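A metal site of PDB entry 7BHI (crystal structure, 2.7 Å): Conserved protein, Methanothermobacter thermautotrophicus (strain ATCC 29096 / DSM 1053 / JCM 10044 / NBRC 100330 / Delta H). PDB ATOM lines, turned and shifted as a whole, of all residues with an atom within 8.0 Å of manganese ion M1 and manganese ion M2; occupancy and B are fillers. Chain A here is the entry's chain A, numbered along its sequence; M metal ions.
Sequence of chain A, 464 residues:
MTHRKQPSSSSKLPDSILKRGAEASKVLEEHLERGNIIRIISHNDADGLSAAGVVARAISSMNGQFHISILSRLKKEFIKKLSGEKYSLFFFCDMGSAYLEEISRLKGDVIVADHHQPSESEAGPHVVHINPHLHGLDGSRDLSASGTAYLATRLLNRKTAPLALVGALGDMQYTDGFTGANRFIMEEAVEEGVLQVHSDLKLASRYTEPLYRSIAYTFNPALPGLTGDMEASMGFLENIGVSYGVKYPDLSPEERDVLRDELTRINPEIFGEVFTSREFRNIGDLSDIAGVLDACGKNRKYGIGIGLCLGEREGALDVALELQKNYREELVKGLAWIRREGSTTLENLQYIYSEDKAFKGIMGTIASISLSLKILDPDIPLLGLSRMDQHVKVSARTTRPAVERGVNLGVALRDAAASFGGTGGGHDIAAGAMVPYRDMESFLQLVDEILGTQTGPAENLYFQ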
ATOM      1  N   SER A  42       5.788  10.659  25.174  1.00  0.00           N
ATOM      2  CA  SER A  42       4.730   9.824  25.731  1.00  0.00           C
ATOM      3  C   SER A  42       4.808   8.394  25.262  1.00  0.00           C
ATOM      4  O   SER A  42       5.576   8.035  24.381  1.00  0.00           O
ATOM      5  CB  SER A  42       3.364  10.446  25.383  1.00  0.00           C
ATOM      6  OG  SER A  42       2.335   9.830  26.120  1.00  0.00           O
ATOM      7  N   HIS A  43       3.975   7.572  25.896  1.00  0.00           N
ATOM      8  CA  HIS A  43       3.934   6.140  25.699  1.00  0.00           C
ATOM      9  C   HIS A  43       3.024   5.788  24.513  1.00  0.00           C
ATOM     10  O   HIS A  43       2.298   6.653  24.024  1.00  0.00           O
ATOM     11  CB  HIS A  43       3.428   5.517  26.999  1.00  0.00           C
ATOM     12  CG  HIS A  43       3.736   4.068  27.123  1.00  0.00           C
ATOM     13  ND1 HIS A  43       2.783   3.152  27.516  1.00  0.00           N
ATOM     14  CD2 HIS A  43       4.876   3.365  26.899  1.00  0.00           C
ATOM     15  CE1 HIS A  43       3.320   1.950  27.517  1.00  0.00           C
ATOM     16  NE2 HIS A  43       4.586   2.046  27.138  1.00  0.00           N
ATOM     17  N   ASN A  44       3.064   4.526  24.088  1.00  0.00           N
ATOM     18  CA  ASN A  44       2.502   4.106  22.801  1.00  0.00           C
ATOM     19  C   ASN A  44       1.239   3.238  22.853  1.00  0.00           C
ATOM     20  O   ASN A  44       1.021   2.400  21.968  1.00  0.00           O
ATOM     21  CB  ASN A  44       3.587   3.376  21.993  1.00  0.00           C
ATOM     22  CG  ASN A  44       3.867   1.951  22.467  1.00  0.00           C
ATOM     23  OD1 ASN A  44       3.504   1.554  23.558  1.00  0.00           O
ATOM     24  ND2 ASN A  44       4.537   1.187  21.631  1.00  0.00           N
ATOM     25  N   ASP A  45       0.437   3.431  23.897  1.00  0.00           N
ATOM     26  CA  ASP A  45      -0.909   2.848  23.995  1.00  0.00           C
ATOM     27  C   ASP A  45      -1.963   3.974  24.133  1.00  0.00           C
ATOM     28  O   ASP A  45      -1.615   5.151  24.151  1.00  0.00           O
ATOM     29  CB  ASP A  45      -0.988   1.808  25.129  1.00  0.00           C
ATOM     30  CG  ASP A  45      -0.422   2.302  26.457  1.00  0.00           C
ATOM     31  OD1 ASP A  45      -0.167   3.522  26.607  1.00  0.00           O
ATOM     32  OD2 ASP A  45      -0.236   1.432  27.369  1.00  0.00           O
ATOM     33  N   ALA A  46      -3.245   3.604  24.213  1.00  0.00           N
ATOM     34  CA  ALA A  46      -4.323   4.573  24.367  1.00  0.00           C
ATOM     35  C   ALA A  46      -4.105   5.657  25.442  1.00  0.00           C
ATOM     36  O   ALA A  46      -4.371   6.810  25.186  1.00  0.00           O
ATOM     37  CB  ALA A  46      -5.636   3.864  24.609  1.00  0.00           C
ATOM     38  N   ASP A  47      -3.608   5.296  26.635  1.00  0.00           N
ATOM     39  CA  ASP A  47      -3.324   6.267  27.715  1.00  0.00           C
ATOM     40  C   ASP A  47      -2.234   7.259  27.341  1.00  0.00           C
ATOM     41  O   ASP A  47      -2.406   8.460  27.479  1.00  0.00           O
ATOM     42  CB  ASP A  47      -2.942   5.534  29.005  1.00  0.00           C
ATOM     43  CG  ASP A  47      -2.800   6.462  30.203  1.00  0.00           C
ATOM     44  OD1 ASP A  47      -3.459   7.515  30.275  1.00  0.00           O
ATOM     45  OD2 ASP A  47      -2.045   6.117  31.147  1.00  0.00           O
ATOM     46  N   GLY A  48      -1.107   6.732  26.876  1.00  0.00           N
ATOM     47  CA  GLY A  48       0.029   7.516  26.407  1.00  0.00           C
ATOM     48  C   GLY A  48      -0.333   8.404  25.229  1.00  0.00           C
ATOM     49  O   GLY A  48      -0.038   9.603  25.248  1.00  0.00           O
ATOM     50  N   LEU A  49      -0.964   7.833  24.207  1.00  0.00           N
ATOM     51  CA  LEU A  49      -1.357   8.608  23.040  1.00  0.00           C
ATOM     52  C   LEU A  49      -2.357   9.707  23.382  1.00  0.00           C
ATOM     53  O   LEU A  49      -2.161  10.867  23.009  1.00  0.00           O
ATOM     54  CB  LEU A  49      -1.968   7.720  21.942  1.00  0.00           C
ATOM     55  CG  LEU A  49      -1.076   6.697  21.239  1.00  0.00           C
ATOM     56  CD1 LEU A  49      -1.933   5.943  20.225  1.00  0.00           C
ATOM     57  CD2 LEU A  49       0.091   7.362  20.547  1.00  0.00           C
ATOM     58  N   ALA A  51      -2.948  11.019  26.307  1.00  0.00           N
ATOM     59  CA  ALA A  51      -2.312  11.993  27.220  1.00  0.00           C
ATOM     60  C   ALA A  51      -1.534  13.086  26.468  1.00  0.00           C
ATOM     61  O   ALA A  51      -1.757  14.265  26.696  1.00  0.00           O
ATOM     62  CB  ALA A  51      -1.391  11.293  28.197  1.00  0.00           C
ATOM     63  N   LEU A  71       7.159   6.585  22.359  1.00  0.00           N
ATOM     64  CA  LEU A  71       8.110   5.495  22.636  1.00  0.00           C
ATOM     65  C   LEU A  71       7.374   4.310  23.224  1.00  0.00           C
ATOM     66  O   LEU A  71       6.368   4.483  23.893  1.00  0.00           O
ATOM     67  CB  LEU A  71       9.137   5.948  23.680  1.00  0.00           C
ATOM     68  CG  LEU A  71       9.772   7.333  23.507  1.00  0.00           C
ATOM     69  CD1 LEU A  71      10.613   7.680  24.735  1.00  0.00           C
ATOM     70  CD2 LEU A  71      10.624   7.373  22.240  1.00  0.00           C
ATOM     71  N   SER A  72       7.886   3.098  22.991  1.00  0.00           N
ATOM     72  CA  SER A  72       7.376   1.899  23.668  1.00  0.00           C
ATOM     73  C   SER A  72       7.901   1.826  25.105  1.00  0.00           C
ATOM     74  O   SER A  72       7.190   1.422  26.021  1.00  0.00           O
ATOM     75  CB  SER A  72       7.771   0.645  22.921  1.00  0.00           C
ATOM     76  OG  SER A  72       9.163   0.461  22.951  1.00  0.00           O
ATOM     77  N   CYS A  93       4.557  12.001  29.519  1.00  0.00           N
ATOM     78  CA  CYS A  93       3.295  11.378  29.925  1.00  0.00           C
ATOM     79  C   CYS A  93       3.414   9.866  30.010  1.00  0.00           C
ATOM     80  O   CYS A  93       4.045   9.238  29.164  1.00  0.00           O
ATOM     81  CB  CYS A  93       2.188  11.735  28.963  1.00  0.00           C
ATOM     82  SG  CYS A  93       1.974  13.515  28.738  1.00  0.00           S
ATOM     83  N   ASP A  94       2.807   9.303  31.046  1.00  0.00           N
ATOM     84  CA  ASP A  94       2.682   7.861  31.246  1.00  0.00           C
ATOM     85  C   ASP A  94       4.031   7.178  31.433  1.00  0.00           C
ATOM     86  O   ASP A  94       4.140   5.957  31.273  1.00  0.00           O
ATOM     87  CB  ASP A  94       1.924   7.259  30.053  1.00  0.00           C
ATOM     88  CG  ASP A  94       1.177   5.988  30.392  1.00  0.00           C
ATOM     89  OD1 ASP A  94       0.904   5.688  31.583  1.00  0.00           O
ATOM     90  OD2 ASP A  94       0.856   5.283  29.414  1.00  0.00           O
ATOM     91  N   MET A  95       5.051   7.963  31.802  1.00  0.00           N
ATOM     92  CA  MET A  95       6.405   7.505  32.051  1.00  0.00           C
ATOM     93  C   MET A  95       7.201   8.680  32.618  1.00  0.00           C
ATOM     94  O   MET A  95       6.912   9.821  32.304  1.00  0.00           O
ATOM     95  CB  MET A  95       7.060   6.970  30.773  1.00  0.00           C
ATOM     96  CG  MET A  95       7.289   8.007  29.687  1.00  0.00           C
ATOM     97  SD  MET A  95       7.502   7.299  28.036  1.00  0.00           S
ATOM     98  CE  MET A  95       8.090   8.758  27.210  1.00  0.00           C
ATOM     99  N   ALA A 113       3.998  13.721  34.039  1.00  0.00           N
ATOM    100  CA  ALA A 113       2.625  13.305  34.278  1.00  0.00           C
ATOM    101  C   ALA A 113       2.477  11.782  34.074  1.00  0.00           C
ATOM    102  O   ALA A 113       2.068  11.331  33.011  1.00  0.00           O
ATOM    103  CB  ALA A 113       1.691  14.078  33.357  1.00  0.00           C
ATOM    104  N   ASP A 114       2.794  11.023  35.115  1.00  0.00           N
ATOM    105  CA  ASP A 114       2.743   9.564  35.142  1.00  0.00           C
ATOM    106  C   ASP A 114       1.712   9.093  36.204  1.00  0.00           C
ATOM    107  O   ASP A 114       1.069   9.903  36.888  1.00  0.00           O
ATOM    108  CB  ASP A 114       4.146   9.082  35.501  1.00  0.00           C
ATOM    109  CG  ASP A 114       4.439   7.630  35.122  1.00  0.00           C
ATOM    110  OD1 ASP A 114       3.513   6.823  34.800  1.00  0.00           O
ATOM    111  OD2 ASP A 114       5.640   7.263  35.159  1.00  0.00           O
ATOM    112  N   HIS A 115       1.490   7.789  36.288  1.00  0.00           N
ATOM    113  CA  HIS A 115       0.671   7.179  37.323  1.00  0.00           C
ATOM    114  C   HIS A 115       1.192   5.811  37.786  1.00  0.00           C
ATOM    115  O   HIS A 115       0.454   5.095  38.442  1.00  0.00           O
ATOM    116  CB  HIS A 115      -0.779   7.071  36.858  1.00  0.00           C
ATOM    117  CG  HIS A 115      -1.002   6.140  35.710  1.00  0.00           C
ATOM    118  ND1 HIS A 115      -1.901   5.082  35.764  1.00  0.00           N
ATOM    119  CD2 HIS A 115      -0.465   6.104  34.468  1.00  0.00           C
ATOM    120  CE1 HIS A 115      -1.884   4.433  34.617  1.00  0.00           C
ATOM    121  NE2 HIS A 115      -1.022   5.041  33.809  1.00  0.00           N
ATOM    122  N   HIS A 116       2.442   5.461  37.490  1.00  0.00           N
ATOM    123  CA  HIS A 116       3.030   4.175  37.875  1.00  0.00           C
ATOM    124  C   HIS A 116       3.710   4.326  39.230  1.00  0.00           C
ATOM    125  O   HIS A 116       3.968   5.461  39.663  1.00  0.00           O
ATOM    126  CB  HIS A 116       4.053   3.722  36.827  1.00  0.00           C
ATOM    127  CG  HIS A 116       3.459   3.419  35.494  1.00  0.00           C
ATOM    128  ND1 HIS A 116       3.885   4.020  34.335  1.00  0.00           N
ATOM    129  CD2 HIS A 116       2.435   2.604  35.144  1.00  0.00           C
ATOM    130  CE1 HIS A 116       3.159   3.565  33.316  1.00  0.00           C
ATOM    131  NE2 HIS A 116       2.279   2.710  33.784  1.00  0.00           N
ATOM    132  N   GLY A 139      -3.290   4.943  41.441  1.00  0.00           N
ATOM    133  CA  GLY A 139      -2.968   5.100  40.025  1.00  0.00           C
ATOM    134  C   GLY A 139      -3.262   3.891  39.139  1.00  0.00           C
ATOM    135  O   GLY A 139      -3.063   3.973  37.937  1.00  0.00           O
ATOM    136  N   LEU A 143      -6.876   6.881  38.291  1.00  0.00           N
ATOM    137  CA  LEU A 143      -6.282   7.965  37.497  1.00  0.00           C
ATOM    138  C   LEU A 143      -5.152   7.453  36.600  1.00  0.00           C
ATOM    139  O   LEU A 143      -4.207   6.805  37.070  1.00  0.00           O
ATOM    140  CB  LEU A 143      -5.772   9.096  38.403  1.00  0.00           C
ATOM    141  CG  LEU A 143      -5.316  10.390  37.734  1.00  0.00           C
ATOM    142  CD1 LEU A 143      -6.443  11.065  36.984  1.00  0.00           C
ATOM    143  CD2 LEU A 143      -4.719  11.338  38.745  1.00  0.00           C
ATOM    144  N   SER A 144      -5.261   7.739  35.305  1.00  0.00           N
ATOM    145  CA  SER A 144      -4.257   7.381  34.294  1.00  0.00           C
ATOM    146  C   SER A 144      -3.458   8.611  33.866  1.00  0.00           C
ATOM    147  O   SER A 144      -3.753   9.744  34.282  1.00  0.00           O
ATOM    148  CB  SER A 144      -4.945   6.734  33.082  1.00  0.00           C
ATOM    149  OG  SER A 144      -5.503   7.697  32.210  1.00  0.00           O
ATOM    150  N   ALA A 145      -2.439   8.373  33.042  1.00  0.00           N
ATOM    151  CA  ALA A 145      -1.590   9.459  32.551  1.00  0.00           C
ATOM    152  C   ALA A 145      -2.410  10.546  31.876  1.00  0.00           C
ATOM    153  O   ALA A 145      -2.108  11.716  32.000  1.00  0.00           O
ATOM    154  CB  ALA A 145      -0.552   8.922  31.575  1.00  0.00           C
ATOM    155  N   SER A 146      -3.432  10.145  31.127  1.00  0.00           N
ATOM    156  CA  SER A 146      -4.266  11.100  30.405  1.00  0.00           C
ATOM    157  C   SER A 146      -4.999  12.070  31.351  1.00  0.00           C
ATOM    158  O   SER A 146      -5.000  13.271  31.111  1.00  0.00           O
ATOM    159  CB  SER A 146      -5.249  10.341  29.505  1.00  0.00           C
ATOM    160  OG  SER A 146      -6.196   9.694  30.304  1.00  0.00           O
ATOM    161  N   GLY A 167      -7.941   7.549  27.691  1.00  0.00           N
ATOM    162  CA  GLY A 167      -6.776   6.939  28.311  1.00  0.00           C
ATOM    163  C   GLY A 167      -7.131   6.088  29.499  1.00  0.00           C
ATOM    164  O   GLY A 167      -6.591   4.988  29.650  1.00  0.00           O
ATOM    165  N   ALA A 168      -8.059   6.581  30.342  1.00  0.00           N
ATOM    166  CA  ALA A 168      -8.591   5.850  31.499  1.00  0.00           C
ATOM    167  C   ALA A 168      -9.162   4.516  31.080  1.00  0.00           C
ATOM    168  O   ALA A 168      -8.794   3.476  31.636  1.00  0.00           O
ATOM    169  CB  ALA A 168      -9.661   6.662  32.201  1.00  0.00           C
ATOM    170  N   GLY A 170      -8.595   3.091  28.231  1.00  0.00           N
ATOM    171  CA  GLY A 170      -7.447   2.403  27.639  1.00  0.00           C
ATOM    172  C   GLY A 170      -6.751   1.484  28.613  1.00  0.00           C
ATOM    173  O   GLY A 170      -6.529   0.323  28.308  1.00  0.00           O
ATOM    174  N   ASP A 171      -6.464   2.007  29.804  1.00  0.00           N
ATOM    175  CA  ASP A 171      -5.846   1.245  30.885  1.00  0.00           C
ATOM    176  C   ASP A 171      -6.867   0.578  31.845  1.00  0.00           C
ATOM    177  O   ASP A 171      -6.540   0.282  32.988  1.00  0.00           O
ATOM    178  CB  ASP A 171      -4.880   2.153  31.669  1.00  0.00           C
ATOM    179  CG  ASP A 171      -3.600   2.471  30.897  1.00  0.00           C
ATOM    180  OD1 ASP A 171      -3.456   2.033  29.724  1.00  0.00           O
ATOM    181  OD2 ASP A 171      -2.720   3.143  31.486  1.00  0.00           O
ATOM    182  N   GLN A 173      -9.357   1.427  33.782  1.00  0.00           N
ATOM    183  CA  GLN A 173      -9.720   2.044  35.050  1.00  0.00           C
ATOM    184  C   GLN A 173     -11.250   2.252  35.144  1.00  0.00           C
ATOM    185  O   GLN A 173     -11.746   3.310  35.549  1.00  0.00           O
ATOM    186  CB  GLN A 173      -9.006   3.371  35.212  1.00  0.00           C
ATOM    187  CG  GLN A 173      -7.514   3.279  35.050  1.00  0.00           C
ATOM    188  CD  GLN A 173      -6.783   4.480  35.627  1.00  0.00           C
ATOM    189  OE1 GLN A 173      -7.316   5.580  35.674  1.00  0.00           O
ATOM    190  NE2 GLN A 173      -5.555   4.260  36.074  1.00  0.00           N
ATOM    191  N   ASP A 294      -5.450   2.166  20.492  1.00  0.00           N
ATOM    192  CA  ASP A 294      -4.629   0.984  20.833  1.00  0.00           C
ATOM    193  C   ASP A 294      -4.166   0.279  19.571  1.00  0.00           C
ATOM    194  O   ASP A 294      -2.985  -0.049  19.427  1.00  0.00           O
ATOM    195  CB  ASP A 294      -5.403  -0.019  21.728  1.00  0.00           C
ATOM    196  CG  ASP A 294      -5.305   0.309  23.230  1.00  0.00           C
ATOM    197  OD1 ASP A 294      -4.192   0.663  23.726  1.00  0.00           O
ATOM    198  OD2 ASP A 294      -6.338   0.197  23.925  1.00  0.00           O
HETATM  199 MN    MN M   1       0.525   3.255  28.949  1.00  0.00          MN
HETATM  200 MN    MN M   2      -0.912   4.370  31.594  1.00  0.00          MN
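Of the 29 residues printed, 4 come within 4 Å of manganese ion M2.
Manganese ion M2 is bound by OD2 of Asp 47 (2.1 Å), OD2 of Asp 171 (2.2 Å), OD1 of Asp 94 (2.2 Å) and NE2 of His 115 (2.3 Å).
Within 4 Å of manganese ion M1: His 43, Asp 45 and Asp 94. The nearest printed residue that does not touch manganese ion M1 is Asp 171 (4.1 Å).
OD2 of Asp 94 is bound to manganese ion M1. Manganese ion M1 is bound by OD1 of Asp 45 (2.5 Å). Manganese ion M1 is bound by the side-chain carboxylate (OD2) of Asp 45 (2.5 Å). Manganese ion M1 is bound by a ring nitrogen (ND1) of His 43, 2.7 Å away. Manganese ion M1 has four donor atoms within binding distance.
The backbone NH (N) of Asp 94 is in hydrogen-bond range of the backbone carbonyl oxygen (O) of Ala 113 (2.9 Å). OD1 of Asp 47 lies within hydrogen-bond range of OG of Ser 144 (2.8 Å). The side-chain carboxylate of Asp 47 is in hydrogen-bond range of the backbone NH of Ser 146, at 2.8 Å. A ring nitrogen (ND1) of His 115 is in hydrogen-bond range of the backbone carbonyl oxygen (O) of Gly 139, at 2.7 Å. The backbone carbonyl oxygen (O) of Leu 143 lies within hydrogen-bond range of a ring nitrogen (ND1) of His 115, 3.2 Å away. OD1 of Asp 45 lies close to N of Gly 48. The backbone NH (N) of Leu 49 lies within hydrogen-bond range of the backbone carbonyl oxygen (O) of His 43 (3.5 Å). A ring nitrogen (NE2) of His 43 lies within hydrogen-bond range of the backbone carbonyl oxygen (O) of Ser 72 (2.9 Å).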
